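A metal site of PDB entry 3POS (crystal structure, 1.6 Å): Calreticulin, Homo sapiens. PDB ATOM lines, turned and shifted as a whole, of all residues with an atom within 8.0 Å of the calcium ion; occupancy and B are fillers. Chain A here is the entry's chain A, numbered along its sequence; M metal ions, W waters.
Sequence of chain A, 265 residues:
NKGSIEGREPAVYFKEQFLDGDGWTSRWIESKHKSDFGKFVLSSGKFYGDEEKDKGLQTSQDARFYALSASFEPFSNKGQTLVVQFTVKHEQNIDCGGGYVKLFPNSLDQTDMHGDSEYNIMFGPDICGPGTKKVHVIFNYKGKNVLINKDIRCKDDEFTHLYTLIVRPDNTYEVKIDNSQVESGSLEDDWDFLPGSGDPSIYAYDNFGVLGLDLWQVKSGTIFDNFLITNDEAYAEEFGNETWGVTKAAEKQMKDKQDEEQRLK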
ATOM      1  N   GLU A  16      -0.685  16.396 -10.540  1.00  0.00           N
ATOM      2  CA  GLU A  16      -0.893  15.078  -9.966  1.00  0.00           C
ATOM      3  C   GLU A  16      -1.747  15.209  -8.738  1.00  0.00           C
ATOM      4  O   GLU A  16      -1.326  15.872  -7.771  1.00  0.00           O
ATOM      5  CB  GLU A  16       0.437  14.377  -9.631  1.00  0.00           C
ATOM      6  CG  GLU A  16       0.214  13.013  -9.011  1.00  0.00           C
ATOM      7  CD  GLU A  16      -0.381  11.969  -9.931  1.00  0.00           C
ATOM      8  OE1 GLU A  16       0.395  11.443 -10.752  1.00  0.00           O
ATOM      9  OE2 GLU A  16      -1.605  11.681  -9.843  1.00  0.00           O
ATOM     10  N   GLN A  17      -2.897  14.543  -8.744  1.00  0.00           N
ATOM     11  CA  GLN A  17      -3.851  14.538  -7.619  1.00  0.00           C
ATOM     12  C   GLN A  17      -4.115  13.145  -7.061  1.00  0.00           C
ATOM     13  O   GLN A  17      -4.809  12.994  -6.046  1.00  0.00           O
ATOM     14  CB  GLN A  17      -5.141  15.240  -8.000  1.00  0.00           C
ATOM     15  CG  GLN A  17      -4.961  16.699  -8.354  1.00  0.00           C
ATOM     16  CD  GLN A  17      -6.267  17.263  -8.856  1.00  0.00           C
ATOM     17  OE1 GLN A  17      -6.535  17.309 -10.051  1.00  0.00           O
ATOM     18  NE2 GLN A  17      -7.152  17.599  -7.947  1.00  0.00           N
ATOM     19  N   PHE A  18      -3.610  12.108  -7.734  1.00  0.00           N
ATOM     20  CA  PHE A  18      -3.823  10.715  -7.282  1.00  0.00           C
ATOM     21  C   PHE A  18      -5.290  10.374  -7.160  1.00  0.00           C
ATOM     22  O   PHE A  18      -5.740   9.856  -6.128  1.00  0.00           O
ATOM     23  CB  PHE A  18      -3.063  10.415  -5.972  1.00  0.00           C
ATOM     24  CG  PHE A  18      -1.631  10.881  -5.983  1.00  0.00           C
ATOM     25  CD1 PHE A  18      -0.649  10.126  -6.619  1.00  0.00           C
ATOM     26  CD2 PHE A  18      -1.269  12.097  -5.416  1.00  0.00           C
ATOM     27  CE1 PHE A  18       0.667  10.589  -6.688  1.00  0.00           C
ATOM     28  CE2 PHE A  18       0.038  12.540  -5.484  1.00  0.00           C
ATOM     29  CZ  PHE A  18       0.992  11.801  -6.129  1.00  0.00           C
ATOM     30  N   LEU A  19      -6.039  10.652  -8.254  1.00  0.00           N
ATOM     31  CA  LEU A  19      -7.486  10.428  -8.325  1.00  0.00           C
ATOM     32  C   LEU A  19      -7.917   9.148  -9.030  1.00  0.00           C
ATOM     33  O   LEU A  19      -9.111   8.850  -9.044  1.00  0.00           O
ATOM     34  CB  LEU A  19      -8.185  11.636  -8.955  1.00  0.00           C
ATOM     35  CG  LEU A  19      -8.144  12.937  -8.141  1.00  0.00           C
ATOM     36  CD1 LEU A  19      -8.509  14.120  -9.006  1.00  0.00           C
ATOM     37  CD2 LEU A  19      -9.075  12.887  -6.920  1.00  0.00           C
ATOM     38  N   ASP A  20      -6.952   8.370  -9.562  1.00  0.00           N
ATOM     39  CA  ASP A  20      -7.253   7.123 -10.275  1.00  0.00           C
ATOM     40  C   ASP A  20      -6.727   5.848  -9.588  1.00  0.00           C
ATOM     41  O   ASP A  20      -6.248   4.938 -10.255  1.00  0.00           O
ATOM     42  CB  ASP A  20      -6.798   7.242 -11.728  1.00  0.00           C
ATOM     43  CG  ASP A  20      -5.304   7.419 -11.906  1.00  0.00           C
ATOM     44  OD1 ASP A  20      -4.622   7.752 -10.909  1.00  0.00           O
ATOM     45  OD2 ASP A  20      -4.799   7.204 -13.040  1.00  0.00           O
ATOM     46  N   LEU A  42      -0.080   4.933  -1.295  1.00  0.00           N
ATOM     47  CA  LEU A  42      -1.207   5.829  -1.540  1.00  0.00           C
ATOM     48  C   LEU A  42      -2.163   5.763  -0.361  1.00  0.00           C
ATOM     49  O   LEU A  42      -2.691   4.701  -0.019  1.00  0.00           O
ATOM     50  CB  LEU A  42      -1.936   5.467  -2.844  1.00  0.00           C
ATOM     51  CG  LEU A  42      -3.077   6.405  -3.276  1.00  0.00           C
ATOM     52  CD1 LEU A  42      -2.550   7.735  -3.752  1.00  0.00           C
ATOM     53  CD2 LEU A  42      -3.892   5.781  -4.376  1.00  0.00           C
ATOM     54  N   SER A  43      -2.391   6.917   0.269  1.00  0.00           N
ATOM     55  CA  SER A  43      -3.290   6.972   1.420  1.00  0.00           C
ATOM     56  C   SER A  43      -3.804   8.382   1.682  1.00  0.00           C
ATOM     57  O   SER A  43      -3.112   9.348   1.362  1.00  0.00           O
ATOM     58  CB  SER A  43      -2.540   6.505   2.666  1.00  0.00           C
ATOM     59  OG  SER A  43      -3.462   6.397   3.739  1.00  0.00           O
ATOM     60  N   SER A  44      -4.966   8.510   2.342  1.00  0.00           N
ATOM     61  CA  SER A  44      -5.463   9.827   2.782  1.00  0.00           C
ATOM     62  C   SER A  44      -5.284   9.975   4.306  1.00  0.00           C
ATOM     63  O   SER A  44      -5.718  10.971   4.896  1.00  0.00           O
ATOM     64  CB  SER A  44      -6.905  10.039   2.358  1.00  0.00           C
ATOM     65  OG  SER A  44      -7.705   8.926   2.736  1.00  0.00           O
ATOM     66  N   ASP A  50     -11.661  14.778   2.636  1.00  0.00           N
ATOM     67  CA  ASP A  50     -12.434  13.822   1.848  1.00  0.00           C
ATOM     68  C   ASP A  50     -11.555  12.601   1.647  1.00  0.00           C
ATOM     69  O   ASP A  50     -10.422  12.738   1.152  1.00  0.00           O
ATOM     70  CB  ASP A  50     -12.846  14.440   0.502  1.00  0.00           C
ATOM     71  CG  ASP A  50     -13.678  13.502  -0.353  1.00  0.00           C
ATOM     72  OD1 ASP A  50     -14.931  13.626  -0.318  1.00  0.00           O
ATOM     73  OD2 ASP A  50     -13.090  12.614  -0.993  1.00  0.00           O
ATOM     74  N   GLU A  51     -12.047  11.428   2.025  1.00  0.00           N
ATOM     75  CA  GLU A  51     -11.297  10.188   1.948  1.00  0.00           C
ATOM     76  C   GLU A  51     -10.703   9.918   0.576  1.00  0.00           C
ATOM     77  O   GLU A  51      -9.604   9.376   0.502  1.00  0.00           O
ATOM     78  CB  GLU A  51     -12.156   8.996   2.390  1.00  0.00           C
ATOM     79  CG  GLU A  51     -11.335   7.787   2.800  1.00  0.00           C
ATOM     80  CD  GLU A  51     -12.123   6.575   3.278  1.00  0.00           C
ATOM     81  OE1 GLU A  51     -13.357   6.667   3.436  1.00  0.00           O
ATOM     82  OE2 GLU A  51     -11.468   5.527   3.538  1.00  0.00           O
ATOM     83  N   GLU A  52     -11.397  10.256  -0.491  1.00  0.00           N
ATOM     84  CA  GLU A  52     -10.879   9.980  -1.825  1.00  0.00           C
ATOM     85  C   GLU A  52     -10.015  11.119  -2.360  1.00  0.00           C
ATOM     86  O   GLU A  52      -8.919  10.873  -2.902  1.00  0.00           O
ATOM     87  CB  GLU A  52     -12.024   9.618  -2.796  1.00  0.00           C
ATOM     88  CG  GLU A  52     -11.598   9.333  -4.235  1.00  0.00           C
ATOM     89  CD  GLU A  52     -10.593   8.214  -4.488  1.00  0.00           C
ATOM     90  OE1 GLU A  52     -10.645   7.179  -3.792  1.00  0.00           O
ATOM     91  OE2 GLU A  52      -9.781   8.371  -5.429  1.00  0.00           O
ATOM     92  N   LYS A  53     -10.501  12.366  -2.281  1.00  0.00           N
ATOM     93  CA  LYS A  53      -9.743  13.496  -2.794  1.00  0.00           C
ATOM     94  C   LYS A  53      -8.413  13.676  -2.085  1.00  0.00           C
ATOM     95  O   LYS A  53      -7.433  14.055  -2.725  1.00  0.00           O
ATOM     96  CB  LYS A  53     -10.522  14.803  -2.686  1.00  0.00           C
ATOM     97  CG  LYS A  53     -11.784  14.862  -3.525  1.00  0.00           C
ATOM     98  CD  LYS A  53     -12.401  16.247  -3.410  1.00  0.00           C
ATOM     99  CE  LYS A  53     -13.764  16.331  -4.044  1.00  0.00           C
ATOM    100  NZ  LYS A  53     -14.310  17.715  -3.946  1.00  0.00           N
ATOM    101  N   ASP A  54      -8.378  13.382  -0.781  1.00  0.00           N
ATOM    102  CA  ASP A  54      -7.149  13.590  -0.007  1.00  0.00           C
ATOM    103  C   ASP A  54      -6.140  12.476  -0.057  1.00  0.00           C
ATOM    104  O   ASP A  54      -5.176  12.470   0.705  1.00  0.00           O
ATOM    105  CB  ASP A  54      -7.440  14.095   1.405  1.00  0.00           C
ATOM    106  CG  ASP A  54      -8.051  15.490   1.329  1.00  0.00           C
ATOM    107  OD1 ASP A  54      -7.464  16.356   0.642  1.00  0.00           O
ATOM    108  OD2 ASP A  54      -9.141  15.696   1.895  1.00  0.00           O
ATOM    109  N   LYS A  55      -6.337  11.543  -0.973  1.00  0.00           N
ATOM    110  CA  LYS A  55      -5.338  10.505  -1.183  1.00  0.00           C
ATOM    111  C   LYS A  55      -4.103  11.166  -1.817  1.00  0.00           C
ATOM    112  O   LYS A  55      -4.187  11.964  -2.746  1.00  0.00           O
ATOM    113  CB  LYS A  55      -5.881   9.405  -2.108  1.00  0.00           C
ATOM    114  CG  LYS A  55      -6.889   8.510  -1.411  1.00  0.00           C
ATOM    115  CD  LYS A  55      -7.209   7.245  -2.190  1.00  0.00           C
ATOM    116  CE  LYS A  55      -8.093   6.303  -1.385  1.00  0.00           C
ATOM    117  NZ  LYS A  55      -7.399   5.766  -0.169  1.00  0.00           N
ATOM    118  N   GLY A  56      -2.954  10.829  -1.255  1.00  0.00           N
ATOM    119  CA  GLY A  56      -1.686  11.291  -1.808  1.00  0.00           C
ATOM    120  C   GLY A  56      -0.599  10.288  -1.486  1.00  0.00           C
ATOM    121  O   GLY A  56      -0.910   9.198  -1.025  1.00  0.00           O
ATOM    122  N   LEU A  57       0.667  10.633  -1.787  1.00  0.00           N
ATOM    123  CA  LEU A  57       1.803   9.763  -1.526  1.00  0.00           C
ATOM    124  C   LEU A  57       2.271   9.948  -0.095  1.00  0.00           C
ATOM    125  O   LEU A  57       2.677  11.042   0.287  1.00  0.00           O
ATOM    126  CB  LEU A  57       2.935  10.058  -2.520  1.00  0.00           C
ATOM    127  CG  LEU A  57       2.559   9.689  -3.964  1.00  0.00           C
ATOM    128  CD1 LEU A  57       3.708   9.973  -4.902  1.00  0.00           C
ATOM    129  CD2 LEU A  57       2.145   8.204  -4.097  1.00  0.00           C
ATOM    130  N   THR A  87       0.760  20.125  -1.943  1.00  0.00           N
ATOM    131  CA  THR A  87       0.379  20.168  -0.521  1.00  0.00           C
ATOM    132  C   THR A  87       1.246  19.155   0.208  1.00  0.00           C
ATOM    133  O   THR A  87       1.664  18.141  -0.388  1.00  0.00           O
ATOM    134  CB  THR A  87      -1.131  19.858  -0.320  1.00  0.00           C
ATOM    135  OG1 THR A  87      -1.411  18.612  -0.914  1.00  0.00           O
ATOM    136  CG2 THR A  87      -2.045  20.920  -0.926  1.00  0.00           C
ATOM    137  N   ILE A 223       2.166  13.146   3.960  1.00  0.00           N
ATOM    138  CA  ILE A 223       1.419  12.890   2.722  1.00  0.00           C
ATOM    139  C   ILE A 223       1.618  14.069   1.779  1.00  0.00           C
ATOM    140  O   ILE A 223       1.398  15.226   2.179  1.00  0.00           O
ATOM    141  CB  ILE A 223      -0.098  12.620   2.996  1.00  0.00           C
ATOM    142  CG1 ILE A 223      -0.274  11.497   4.017  1.00  0.00           C
ATOM    143  CG2 ILE A 223      -0.877  12.282   1.664  1.00  0.00           C
ATOM    144  CD1 ILE A 223      -1.731  11.256   4.315  1.00  0.00           C
ATOM    145  N   PHE A 224       1.966  13.768   0.502  1.00  0.00           N
ATOM    146  CA  PHE A 224       2.155  14.792  -0.546  1.00  0.00           C
ATOM    147  C   PHE A 224       1.004  14.645  -1.526  1.00  0.00           C
ATOM    148  O   PHE A 224       0.599  13.514  -1.830  1.00  0.00           O
ATOM    149  CB  PHE A 224       3.480  14.549  -1.317  1.00  0.00           C
ATOM    150  CG  PHE A 224       4.703  14.705  -0.449  1.00  0.00           C
ATOM    151  CD1 PHE A 224       5.308  15.952  -0.290  1.00  0.00           C
ATOM    152  CD2 PHE A 224       5.216  13.625   0.260  1.00  0.00           C
ATOM    153  CE1 PHE A 224       6.454  16.089   0.500  1.00  0.00           C
ATOM    154  CE2 PHE A 224       6.377  13.761   1.049  1.00  0.00           C
ATOM    155  CZ  PHE A 224       6.985  14.990   1.164  1.00  0.00           C
ATOM    156  N   ASP A 225       0.465  15.778  -2.006  1.00  0.00           N
ATOM    157  CA  ASP A 225      -0.681  15.748  -2.924  1.00  0.00           C
ATOM    158  C   ASP A 225      -0.712  16.997  -3.762  1.00  0.00           C
ATOM    159  O   ASP A 225       0.037  17.957  -3.547  1.00  0.00           O
ATOM    160  CB  ASP A 225      -1.993  15.634  -2.102  1.00  0.00           C
ATOM    161  CG  ASP A 225      -3.251  15.108  -2.841  1.00  0.00           C
ATOM    162  OD1 ASP A 225      -3.155  14.803  -4.068  1.00  0.00           O
ATOM    163  OD2 ASP A 225      -4.295  14.906  -2.177  1.00  0.00           O
ATOM    164  N   ASN A 226      -1.612  16.987  -4.747  1.00  0.00           N
ATOM    165  CA  ASN A 226      -1.964  18.178  -5.513  1.00  0.00           C
ATOM    166  C   ASN A 226      -0.790  18.906  -6.077  1.00  0.00           C
ATOM    167  O   ASN A 226      -0.687  20.123  -5.943  1.00  0.00           O
ATOM    168  CB  ASN A 226      -2.842  19.088  -4.610  1.00  0.00           C
ATOM    169  CG  ASN A 226      -4.056  18.354  -4.144  1.00  0.00           C
ATOM    170  OD1 ASN A 226      -4.396  18.343  -2.949  1.00  0.00           O
ATOM    171  ND2 ASN A 226      -4.755  17.745  -5.069  1.00  0.00           N
ATOM    172  N   PHE A 227       0.060  18.164  -6.810  1.00  0.00           N
ATOM    173  CA  PHE A 227       1.208  18.799  -7.435  1.00  0.00           C
ATOM    174  C   PHE A 227       0.746  19.588  -8.647  1.00  0.00           C
ATOM    175  O   PHE A 227      -0.130  19.137  -9.395  1.00  0.00           O
ATOM    176  CB  PHE A 227       2.234  17.755  -7.917  1.00  0.00           C
ATOM    177  CG  PHE A 227       2.906  16.986  -6.793  1.00  0.00           C
ATOM    178  CD1 PHE A 227       4.067  17.464  -6.202  1.00  0.00           C
ATOM    179  CD2 PHE A 227       2.355  15.793  -6.308  1.00  0.00           C
ATOM    180  CE1 PHE A 227       4.715  16.731  -5.177  1.00  0.00           C
ATOM    181  CE2 PHE A 227       2.983  15.073  -5.286  1.00  0.00           C
ATOM    182  CZ  PHE A 227       4.161  15.533  -4.739  1.00  0.00           C
ATOM    183  N   THR A 243      -8.059  22.597  -4.236  1.00  0.00           N
ATOM    184  CA  THR A 243      -7.398  21.453  -3.598  1.00  0.00           C
ATOM    185  C   THR A 243      -7.265  21.682  -2.112  1.00  0.00           C
ATOM    186  O   THR A 243      -8.122  21.232  -1.328  1.00  0.00           O
ATOM    187  CB  THR A 243      -6.076  21.145  -4.332  1.00  0.00           C
ATOM    188  OG1 THR A 243      -5.224  22.307  -4.336  1.00  0.00           O
ATOM    189  CG2 THR A 243      -6.328  20.724  -5.782  1.00  0.00           C
ATOM    190  N   THR A 247      -9.844  20.936   1.214  1.00  0.00           N
ATOM    191  CA  THR A 247      -9.448  20.033   2.278  1.00  0.00           C
ATOM    192  C   THR A 247      -9.568  20.673   3.649  1.00  0.00           C
ATOM    193  O   THR A 247     -10.026  20.019   4.584  1.00  0.00           O
ATOM    194  CB  THR A 247      -7.939  19.656   2.075  1.00  0.00           C
ATOM    195  OG1 THR A 247      -7.806  19.005   0.827  1.00  0.00           O
ATOM    196  CG2 THR A 247      -7.390  18.764   3.191  1.00  0.00           C
HETATM  197 CA    CA M   1      -5.387  13.618  -3.934  1.00  0.00          CA
HETATM  198  O   HOH W   1      -6.344  15.684  -4.744  1.00  0.00           O
HETATM  199  O   HOH W   2      -6.947  11.917  -4.466  1.00  0.00           O
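Water W2 lies within hydrogen-bond range of the backbone carbonyl oxygen (O) of Glu 52 and the backbone carbonyl oxygen (O) of Phe 18.
The calcium ion is bound by O of Gln 17, 2.3 Å away.
O of Lys 55 binds the calcium ion (2.4 Å).
The calcium ion is bound by water W2, at 2.4 Å.
Water W1 is bound to the calcium ion.
The calcium ion is bound by the backbone carbonyl oxygen (O) of Lys 53, 2.4 Å away.
OD2 of Asp 225 is bound to the calcium ion, at 2.4 Å.
OD1 of Asp 225 binds the calcium ion, at 2.5 Å.
The calcium ion has seven donor atoms within binding distance.
Of the 24 residues printed, 4 come within 4 Å of the calcium ion.
The nearest printed residue that does not touch the calcium ion is Asp 54 (4.1 Å).
OD2 of Asp 50 sits at hydrogen-bond distance from N of Lys 53 (2.9 Å).
The side-chain carboxylate (OD1) of Asp 225 sits close to the side-chain amide nitrogen (ND2) of Asn 226 (3.5 Å).
The backbone carbonyl oxygen (O) of Asp 225 sits at hydrogen-bond distance from the backbone NH (N) of Thr 87, 2.8 Å away.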
